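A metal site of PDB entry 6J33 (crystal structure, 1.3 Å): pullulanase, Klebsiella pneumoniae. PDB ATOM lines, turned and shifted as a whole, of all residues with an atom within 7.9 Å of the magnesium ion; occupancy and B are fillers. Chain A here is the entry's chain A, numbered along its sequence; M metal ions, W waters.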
ATOM      1  N   LEU A 354     -10.409  -1.016  31.213  1.00  0.00           N
ATOM      2  CA  LEU A 354      -9.709  -1.921  32.112  1.00  0.00           C
ATOM      3  C   LEU A 354      -8.611  -1.160  32.843  1.00  0.00           C
ATOM      4  O   LEU A 354      -8.107  -0.134  32.384  1.00  0.00           O
ATOM      5  CB  LEU A 354      -9.035  -3.063  31.324  1.00  0.00           C
ATOM      6  CG  LEU A 354      -9.961  -4.061  30.626  1.00  0.00           C
ATOM      7  CD1 LEU A 354      -9.201  -4.847  29.552  1.00  0.00           C
ATOM      8  CD2 LEU A 354     -10.626  -5.000  31.617  1.00  0.00           C
ATOM      9  N   SER A 355      -8.246  -1.679  34.028  1.00  0.00           N
ATOM     10  CA  SER A 355      -7.013  -1.303  34.691  1.00  0.00           C
ATOM     11  C   SER A 355      -5.816  -1.949  34.000  1.00  0.00           C
ATOM     12  O   SER A 355      -5.944  -2.765  33.083  1.00  0.00           O
ATOM     13  CB  SER A 355      -7.032  -1.717  36.162  1.00  0.00           C
ATOM     14  OG  SER A 355      -6.977  -3.118  36.303  1.00  0.00           O
ATOM     15  N   THR A 356      -4.621  -1.577  34.458  1.00  0.00           N
ATOM     16  CA  THR A 356      -3.386  -2.130  33.901  1.00  0.00           C
ATOM     17  C   THR A 356      -3.399  -3.656  33.992  1.00  0.00           C
ATOM     18  O   THR A 356      -3.676  -4.225  35.046  1.00  0.00           O
ATOM     19  CB  THR A 356      -2.179  -1.596  34.681  1.00  0.00           C
ATOM     20  OG1 THR A 356      -2.118  -0.169  34.579  1.00  0.00           O
ATOM     21  CG2 THR A 356      -0.877  -2.194  34.137  1.00  0.00           C
ATOM     22  N   ASN A 357      -3.083  -4.312  32.872  1.00  0.00           N
ATOM     23  CA  ASN A 357      -3.007  -5.765  32.810  1.00  0.00           C
ATOM     24  C   ASN A 357      -4.356  -6.445  33.011  1.00  0.00           C
ATOM     25  O   ASN A 357      -4.400  -7.646  33.288  1.00  0.00           O
ATOM     26  CB  ASN A 357      -1.946  -6.343  33.744  1.00  0.00           C
ATOM     27  CG  ASN A 357      -1.255  -7.553  33.141  1.00  0.00           C
ATOM     28  OD1 ASN A 357      -0.954  -7.577  31.947  1.00  0.00           O
ATOM     29  ND2 ASN A 357      -0.985  -8.561  33.963  1.00  0.00           N
ATOM     30  N   SER A 358      -5.451  -5.699  32.889  1.00  0.00           N
ATOM     31  CA  SER A 358      -6.811  -6.237  32.807  1.00  0.00           C
ATOM     32  C   SER A 358      -7.300  -6.825  34.125  1.00  0.00           C
ATOM     33  O   SER A 358      -8.174  -7.696  34.120  1.00  0.00           O
ATOM     34  CB  SER A 358      -6.942  -7.284  31.699  1.00  0.00           C
ATOM     35  OG  SER A 358      -6.194  -6.907  30.542  1.00  0.00           O
ATOM     36  N   PHE A 450      -7.377  -5.682  20.208  1.00  0.00           N
ATOM     37  CA  PHE A 450      -8.193  -5.903  21.391  1.00  0.00           C
ATOM     38  C   PHE A 450      -7.268  -6.348  22.520  1.00  0.00           C
ATOM     39  O   PHE A 450      -6.056  -6.512  22.324  1.00  0.00           O
ATOM     40  CB  PHE A 450      -9.242  -6.986  21.093  1.00  0.00           C
ATOM     41  CG  PHE A 450      -8.639  -8.258  20.548  1.00  0.00           C
ATOM     42  CD1 PHE A 450      -8.096  -9.206  21.402  1.00  0.00           C
ATOM     43  CD2 PHE A 450      -8.551  -8.464  19.192  1.00  0.00           C
ATOM     44  CE1 PHE A 450      -7.485 -10.348  20.904  1.00  0.00           C
ATOM     45  CE2 PHE A 450      -7.938  -9.608  18.684  1.00  0.00           C
ATOM     46  CZ  PHE A 450      -7.415 -10.543  19.542  1.00  0.00           C
ATOM     47  N   ASP A 451      -7.818  -6.554  23.712  1.00  0.00           N
ATOM     48  CA  ASP A 451      -6.971  -6.788  24.884  1.00  0.00           C
ATOM     49  C   ASP A 451      -6.420  -8.211  24.861  1.00  0.00           C
ATOM     50  O   ASP A 451      -7.149  -9.173  25.103  1.00  0.00           O
ATOM     51  CB  ASP A 451      -7.743  -6.573  26.182  1.00  0.00           C
ATOM     52  CG  ASP A 451      -6.914  -6.918  27.405  1.00  0.00           C
ATOM     53  OD1 ASP A 451      -5.686  -6.659  27.393  1.00  0.00           O
ATOM     54  OD2 ASP A 451      -7.498  -7.461  28.370  1.00  0.00           O
ATOM     55  N   LEU A 452      -5.139  -8.344  24.547  1.00  0.00           N
ATOM     56  CA  LEU A 452      -4.520  -9.663  24.568  1.00  0.00           C
ATOM     57  C   LEU A 452      -3.959  -9.959  25.955  1.00  0.00           C
ATOM     58  O   LEU A 452      -3.773  -9.056  26.771  1.00  0.00           O
ATOM     59  CB  LEU A 452      -3.439  -9.767  23.488  1.00  0.00           C
ATOM     60  CG  LEU A 452      -2.448  -8.606  23.466  1.00  0.00           C
ATOM     61  CD1 LEU A 452      -1.065  -9.056  23.907  1.00  0.00           C
ATOM     62  CD2 LEU A 452      -2.395  -7.930  22.103  1.00  0.00           C
ATOM     63  N   ALA A 453      -3.715 -11.237  26.203  1.00  0.00           N
ATOM     64  CA  ALA A 453      -3.305 -11.736  27.519  1.00  0.00           C
ATOM     65  C   ALA A 453      -1.796 -11.879  27.702  1.00  0.00           C
ATOM     66  O   ALA A 453      -1.321 -11.783  28.843  1.00  0.00           O
ATOM     67  CB  ALA A 453      -3.942 -13.091  27.790  1.00  0.00           C
ATOM     68  N   THR A 454      -1.050 -12.102  26.620  1.00  0.00           N
ATOM     69  CA  THR A 454       0.306 -12.671  26.633  1.00  0.00           C
ATOM     70  C   THR A 454       1.428 -11.644  26.625  1.00  0.00           C
ATOM     71  O   THR A 454       2.578 -11.995  26.330  1.00  0.00           O
ATOM     72  CB  THR A 454       0.467 -13.602  25.435  1.00  0.00           C
ATOM     73  OG1 THR A 454      -0.100 -12.998  24.263  1.00  0.00           O
ATOM     74  CG2 THR A 454      -0.219 -14.899  25.715  1.00  0.00           C
ATOM     75  N   VAL A 455       1.119 -10.393  26.901  1.00  0.00           N
ATOM     76  CA  VAL A 455       2.101  -9.375  27.251  1.00  0.00           C
ATOM     77  C   VAL A 455       1.688  -8.818  28.602  1.00  0.00           C
ATOM     78  O   VAL A 455       0.497  -8.538  28.830  1.00  0.00           O
ATOM     79  CB  VAL A 455       2.147  -8.261  26.191  1.00  0.00           C
ATOM     80  CG1 VAL A 455       3.008  -7.115  26.666  1.00  0.00           C
ATOM     81  CG2 VAL A 455       2.680  -8.806  24.862  1.00  0.00           C
ATOM     82  N   ASN A 456       2.647  -8.674  29.508  1.00  0.00           N
ATOM     83  CA  ASN A 456       2.362  -8.070  30.802  1.00  0.00           C
ATOM     84  C   ASN A 456       2.319  -6.552  30.638  1.00  0.00           C
ATOM     85  O   ASN A 456       3.293  -5.947  30.157  1.00  0.00           O
ATOM     86  CB  ASN A 456       3.403  -8.506  31.827  1.00  0.00           C
ATOM     87  CG  ASN A 456       2.946  -8.240  33.241  1.00  0.00           C
ATOM     88  OD1 ASN A 456       2.375  -7.194  33.528  1.00  0.00           O
ATOM     89  ND2 ASN A 456       3.205  -9.192  34.132  1.00  0.00           N
ATOM     90  N   GLU A 457       1.201  -5.935  31.008  1.00  0.00           N
ATOM     91  CA  GLU A 457       1.043  -4.499  30.828  1.00  0.00           C
ATOM     92  C   GLU A 457       1.667  -3.693  31.963  1.00  0.00           C
ATOM     93  O   GLU A 457       1.715  -2.470  31.860  1.00  0.00           O
ATOM     94  CB  GLU A 457      -0.438  -4.149  30.669  1.00  0.00           C
ATOM     95  CG  GLU A 457      -1.093  -4.884  29.512  1.00  0.00           C
ATOM     96  CD  GLU A 457      -2.548  -4.498  29.289  1.00  0.00           C
ATOM     97  OE1 GLU A 457      -3.122  -3.738  30.115  1.00  0.00           O
ATOM     98  OE2 GLU A 457      -3.134  -4.948  28.273  1.00  0.00           O
ATOM     99  N   ASP A 530      -4.579 -14.113  21.537  1.00  0.00           N
ATOM    100  CA  ASP A 530      -4.724 -14.638  22.891  1.00  0.00           C
ATOM    101  C   ASP A 530      -5.709 -13.740  23.625  1.00  0.00           C
ATOM    102  O   ASP A 530      -5.325 -12.940  24.493  1.00  0.00           O
ATOM    103  CB  ASP A 530      -3.376 -14.651  23.618  1.00  0.00           C
ATOM    104  CG  ASP A 530      -2.335 -15.417  22.858  1.00  0.00           C
ATOM    105  OD1 ASP A 530      -2.534 -16.641  22.712  1.00  0.00           O
ATOM    106  OD2 ASP A 530      -1.331 -14.794  22.431  1.00  0.00           O
ATOM    107  N   PRO A 531      -6.999 -13.851  23.300  1.00  0.00           N
ATOM    108  CA  PRO A 531      -7.956 -12.826  23.752  1.00  0.00           C
ATOM    109  C   PRO A 531      -8.208 -12.923  25.253  1.00  0.00           C
ATOM    110  O   PRO A 531      -8.535 -13.984  25.787  1.00  0.00           O
ATOM    111  CB  PRO A 531      -9.230 -13.149  22.965  1.00  0.00           C
ATOM    112  CG  PRO A 531      -8.851 -14.177  21.968  1.00  0.00           C
ATOM    113  CD  PRO A 531      -7.599 -14.833  22.384  1.00  0.00           C
ATOM    114  N   PHE A 532      -8.075 -11.777  25.914  1.00  0.00           N
ATOM    115  CA  PHE A 532      -8.432 -11.606  27.316  1.00  0.00           C
ATOM    116  C   PHE A 532      -9.767 -10.901  27.435  1.00  0.00           C
ATOM    117  O   PHE A 532     -10.666 -11.403  28.118  1.00  0.00           O
ATOM    118  CB  PHE A 532      -7.305 -10.823  28.017  1.00  0.00           C
ATOM    119  CG  PHE A 532      -7.214 -10.996  29.522  1.00  0.00           C
ATOM    120  CD1 PHE A 532      -8.192 -11.635  30.249  1.00  0.00           C
ATOM    121  CD2 PHE A 532      -6.107 -10.483  30.192  1.00  0.00           C
ATOM    122  CE1 PHE A 532      -8.072 -11.762  31.635  1.00  0.00           C
ATOM    123  CE2 PHE A 532      -5.972 -10.595  31.557  1.00  0.00           C
ATOM    124  CZ  PHE A 532      -6.951 -11.244  32.286  1.00  0.00           C
ATOM    125  N   HIS A 533      -9.938  -9.763  26.762  1.00  0.00           N
ATOM    126  CA  HIS A 533     -11.228  -9.083  26.667  1.00  0.00           C
ATOM    127  C   HIS A 533     -11.418  -8.652  25.223  1.00  0.00           C
ATOM    128  O   HIS A 533     -10.512  -8.053  24.625  1.00  0.00           O
ATOM    129  CB  HIS A 533     -11.307  -7.871  27.613  1.00  0.00           C
ATOM    130  CG  HIS A 533     -11.173  -8.245  29.054  1.00  0.00           C
ATOM    131  ND1 HIS A 533      -9.944  -8.442  29.661  1.00  0.00           N
ATOM    132  CD2 HIS A 533     -12.104  -8.542  29.990  1.00  0.00           C
ATOM    133  CE1 HIS A 533     -10.139  -8.807  30.918  1.00  0.00           C
ATOM    134  NE2 HIS A 533     -11.445  -8.882  31.146  1.00  0.00           N
ATOM    135  N   VAL A 536     -12.076  -4.198  24.498  1.00  0.00           N
ATOM    136  CA  VAL A 536     -11.233  -3.132  25.029  1.00  0.00           C
ATOM    137  C   VAL A 536      -9.931  -3.133  24.232  1.00  0.00           C
ATOM    138  O   VAL A 536      -9.418  -4.208  23.919  1.00  0.00           O
ATOM    139  CB  VAL A 536     -10.875  -3.366  26.517  1.00  0.00           C
ATOM    140  CG1 VAL A 536     -10.220  -2.135  27.110  1.00  0.00           C
ATOM    141  CG2 VAL A 536     -12.101  -3.782  27.313  1.00  0.00           C
ATOM    142  N   PRO A 537      -9.356  -1.976  23.907  1.00  0.00           N
ATOM    143  CA  PRO A 537      -8.021  -1.979  23.285  1.00  0.00           C
ATOM    144  C   PRO A 537      -6.978  -2.598  24.203  1.00  0.00           C
ATOM    145  O   PRO A 537      -7.080  -2.548  25.433  1.00  0.00           O
ATOM    146  CB  PRO A 537      -7.741  -0.487  23.047  1.00  0.00           C
ATOM    147  CG  PRO A 537      -9.096   0.137  22.949  1.00  0.00           C
ATOM    148  CD  PRO A 537      -9.938  -0.616  23.958  1.00  0.00           C
ATOM    149  N   GLU A 538      -5.946  -3.162  23.586  1.00  0.00           N
ATOM    150  CA  GLU A 538      -4.798  -3.671  24.336  1.00  0.00           C
ATOM    151  C   GLU A 538      -4.100  -2.538  25.083  1.00  0.00           C
ATOM    152  O   GLU A 538      -3.918  -1.438  24.564  1.00  0.00           O
ATOM    153  CB  GLU A 538      -3.837  -4.348  23.352  1.00  0.00           C
ATOM    154  CG  GLU A 538      -2.423  -4.596  23.851  1.00  0.00           C
ATOM    155  CD  GLU A 538      -2.337  -5.465  25.085  1.00  0.00           C
ATOM    156  OE1 GLU A 538      -1.235  -5.522  25.657  1.00  0.00           O
ATOM    157  OE2 GLU A 538      -3.341  -6.087  25.511  1.00  0.00           O
ATOM    158  N   GLY A 539      -3.704  -2.823  26.330  1.00  0.00           N
ATOM    159  CA  GLY A 539      -3.079  -1.801  27.148  1.00  0.00           C
ATOM    160  C   GLY A 539      -1.617  -1.526  26.869  1.00  0.00           C
ATOM    161  O   GLY A 539      -1.172  -0.393  26.991  1.00  0.00           O
ATOM    162  N   SER A 540      -0.856  -2.552  26.470  1.00  0.00           N
ATOM    163  CA  SER A 540       0.582  -2.361  26.329  1.00  0.00           C
ATOM    164  C   SER A 540       0.935  -1.464  25.158  1.00  0.00           C
ATOM    165  O   SER A 540       2.045  -0.924  25.115  1.00  0.00           O
ATOM    166  CB  SER A 540       1.310  -3.706  26.221  1.00  0.00           C
ATOM    167  OG  SER A 540       1.019  -4.332  24.980  1.00  0.00           O
ATOM    168  N   TYR A 541       0.015  -1.282  24.211  1.00  0.00           N
ATOM    169  CA  TYR A 541       0.227  -0.395  23.076  1.00  0.00           C
ATOM    170  C   TYR A 541      -0.134   1.046  23.406  1.00  0.00           C
ATOM    171  O   TYR A 541       0.034   1.932  22.564  1.00  0.00           O
ATOM    172  CB  TYR A 541      -0.555  -0.892  21.864  1.00  0.00           C
ATOM    173  CG  TYR A 541      -0.176  -2.275  21.370  1.00  0.00           C
ATOM    174  CD1 TYR A 541       1.129  -2.719  21.419  1.00  0.00           C
ATOM    175  CD2 TYR A 541      -1.139  -3.124  20.841  1.00  0.00           C
ATOM    176  CE1 TYR A 541       1.468  -3.989  20.955  1.00  0.00           C
ATOM    177  CE2 TYR A 541      -0.824  -4.389  20.392  1.00  0.00           C
ATOM    178  CZ  TYR A 541       0.483  -4.813  20.437  1.00  0.00           C
ATOM    179  OH  TYR A 541       0.861  -6.064  19.988  1.00  0.00           O
ATOM    180  N   ARG A 550      -6.056   4.604  27.224  1.00  0.00           N
ATOM    181  CA  ARG A 550      -5.794   3.907  25.965  1.00  0.00           C
ATOM    182  C   ARG A 550      -6.897   4.111  24.925  1.00  0.00           C
ATOM    183  O   ARG A 550      -6.636   3.948  23.730  1.00  0.00           O
ATOM    184  CB  ARG A 550      -5.628   2.416  26.232  1.00  0.00           C
ATOM    185  CG  ARG A 550      -6.919   1.727  26.635  1.00  0.00           C
ATOM    186  CD  ARG A 550      -6.714   0.255  26.916  1.00  0.00           C
ATOM    187  NE  ARG A 550      -6.155   0.050  28.242  1.00  0.00           N
ATOM    188  CZ  ARG A 550      -6.117  -1.127  28.853  1.00  0.00           C
ATOM    189  NH1 ARG A 550      -6.588  -2.205  28.256  1.00  0.00           N
ATOM    190  NH2 ARG A 550      -5.658  -1.245  30.099  1.00  0.00           N
ATOM    191  N   ARG A 586      -5.886 -17.220  35.450  1.00  0.00           N
ATOM    192  CA  ARG A 586      -6.025 -15.769  35.469  1.00  0.00           C
ATOM    193  C   ARG A 586      -6.867 -15.235  34.317  1.00  0.00           C
ATOM    194  O   ARG A 586      -7.660 -14.297  34.509  1.00  0.00           O
ATOM    195  CB  ARG A 586      -4.610 -15.161  35.411  1.00  0.00           C
ATOM    196  CG  ARG A 586      -4.547 -13.666  35.180  1.00  0.00           C
ATOM    197  CD  ARG A 586      -3.118 -13.159  35.032  1.00  0.00           C
ATOM    198  NE  ARG A 586      -2.513 -13.517  33.751  1.00  0.00           N
ATOM    199  CZ  ARG A 586      -2.371 -12.671  32.736  1.00  0.00           C
ATOM    200  NH1 ARG A 586      -2.799 -11.417  32.851  1.00  0.00           N
ATOM    201  NH2 ARG A 586      -1.810 -13.069  31.601  1.00  0.00           N
HETATM  202 MG    MG M   1      -3.629  -6.986  27.509  1.00  0.00          MG
HETATM  203  O   HOH W   1      -3.744  -7.643  29.585  1.00  0.00           O
HETATM  204  O   HOH W   2      -1.547  -7.533  27.395  1.00  0.00           O
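The backbone NH (N) of Phe 532 is in hydrogen-bond range of the backbone carbonyl oxygen (O) of Asp 451, 2.9 Å away.
The side-chain carboxylate of Glu 538 lies within hydrogen-bond range of the side-chain hydroxyl of Ser 540 (2.6 Å).
The side-chain carboxylate (OE1) of Glu 457 lies within salt-bridge range of the guanidinium group (NH2) of Arg 550, 3.6 Å away.
ND1 of His 533 sits at hydrogen-bond distance from OD2 of Asp 451 (2.9 Å).
The side-chain carboxylate (OD2) of Asp 451 sits at hydrogen-bond distance from the side-chain hydroxyl (OG) of Ser 358 (2.6 Å).
N of Gly 539 sits close to OE2 of Glu 457, at 2.9 Å.
The backbone NH (N) of Asp 451 lies within hydrogen-bond range of the backbone carbonyl oxygen (O) of Val 536 (2.8 Å).
The side-chain carboxylate of Glu 457 lies within hydrogen-bond range of the backbone NH of Asn 357.
Residues that only touch the magnesium ion: Ser 358 (3.97 Å).
The nearest printed residue that does not touch the magnesium ion is Gly 539 (4.3 Å).
The magnesium ion is bound by OD1 of Asp 451 (2.1 Å), water W2 (2.2 Å), water W1 (2.2 Å), O of Leu 452 (2.2 Å), OE2 of Glu 538 (2.2 Å) and OE2 of Glu 457 (2.2 Å).
The magnesium ion has six donor atoms within binding distance.
Water W2 lies within hydrogen-bond range of the side-chain carboxylate (OE1) of Glu 538 (2.7 Å) and the backbone carbonyl oxygen (O) of Val 455 (2.7 Å).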
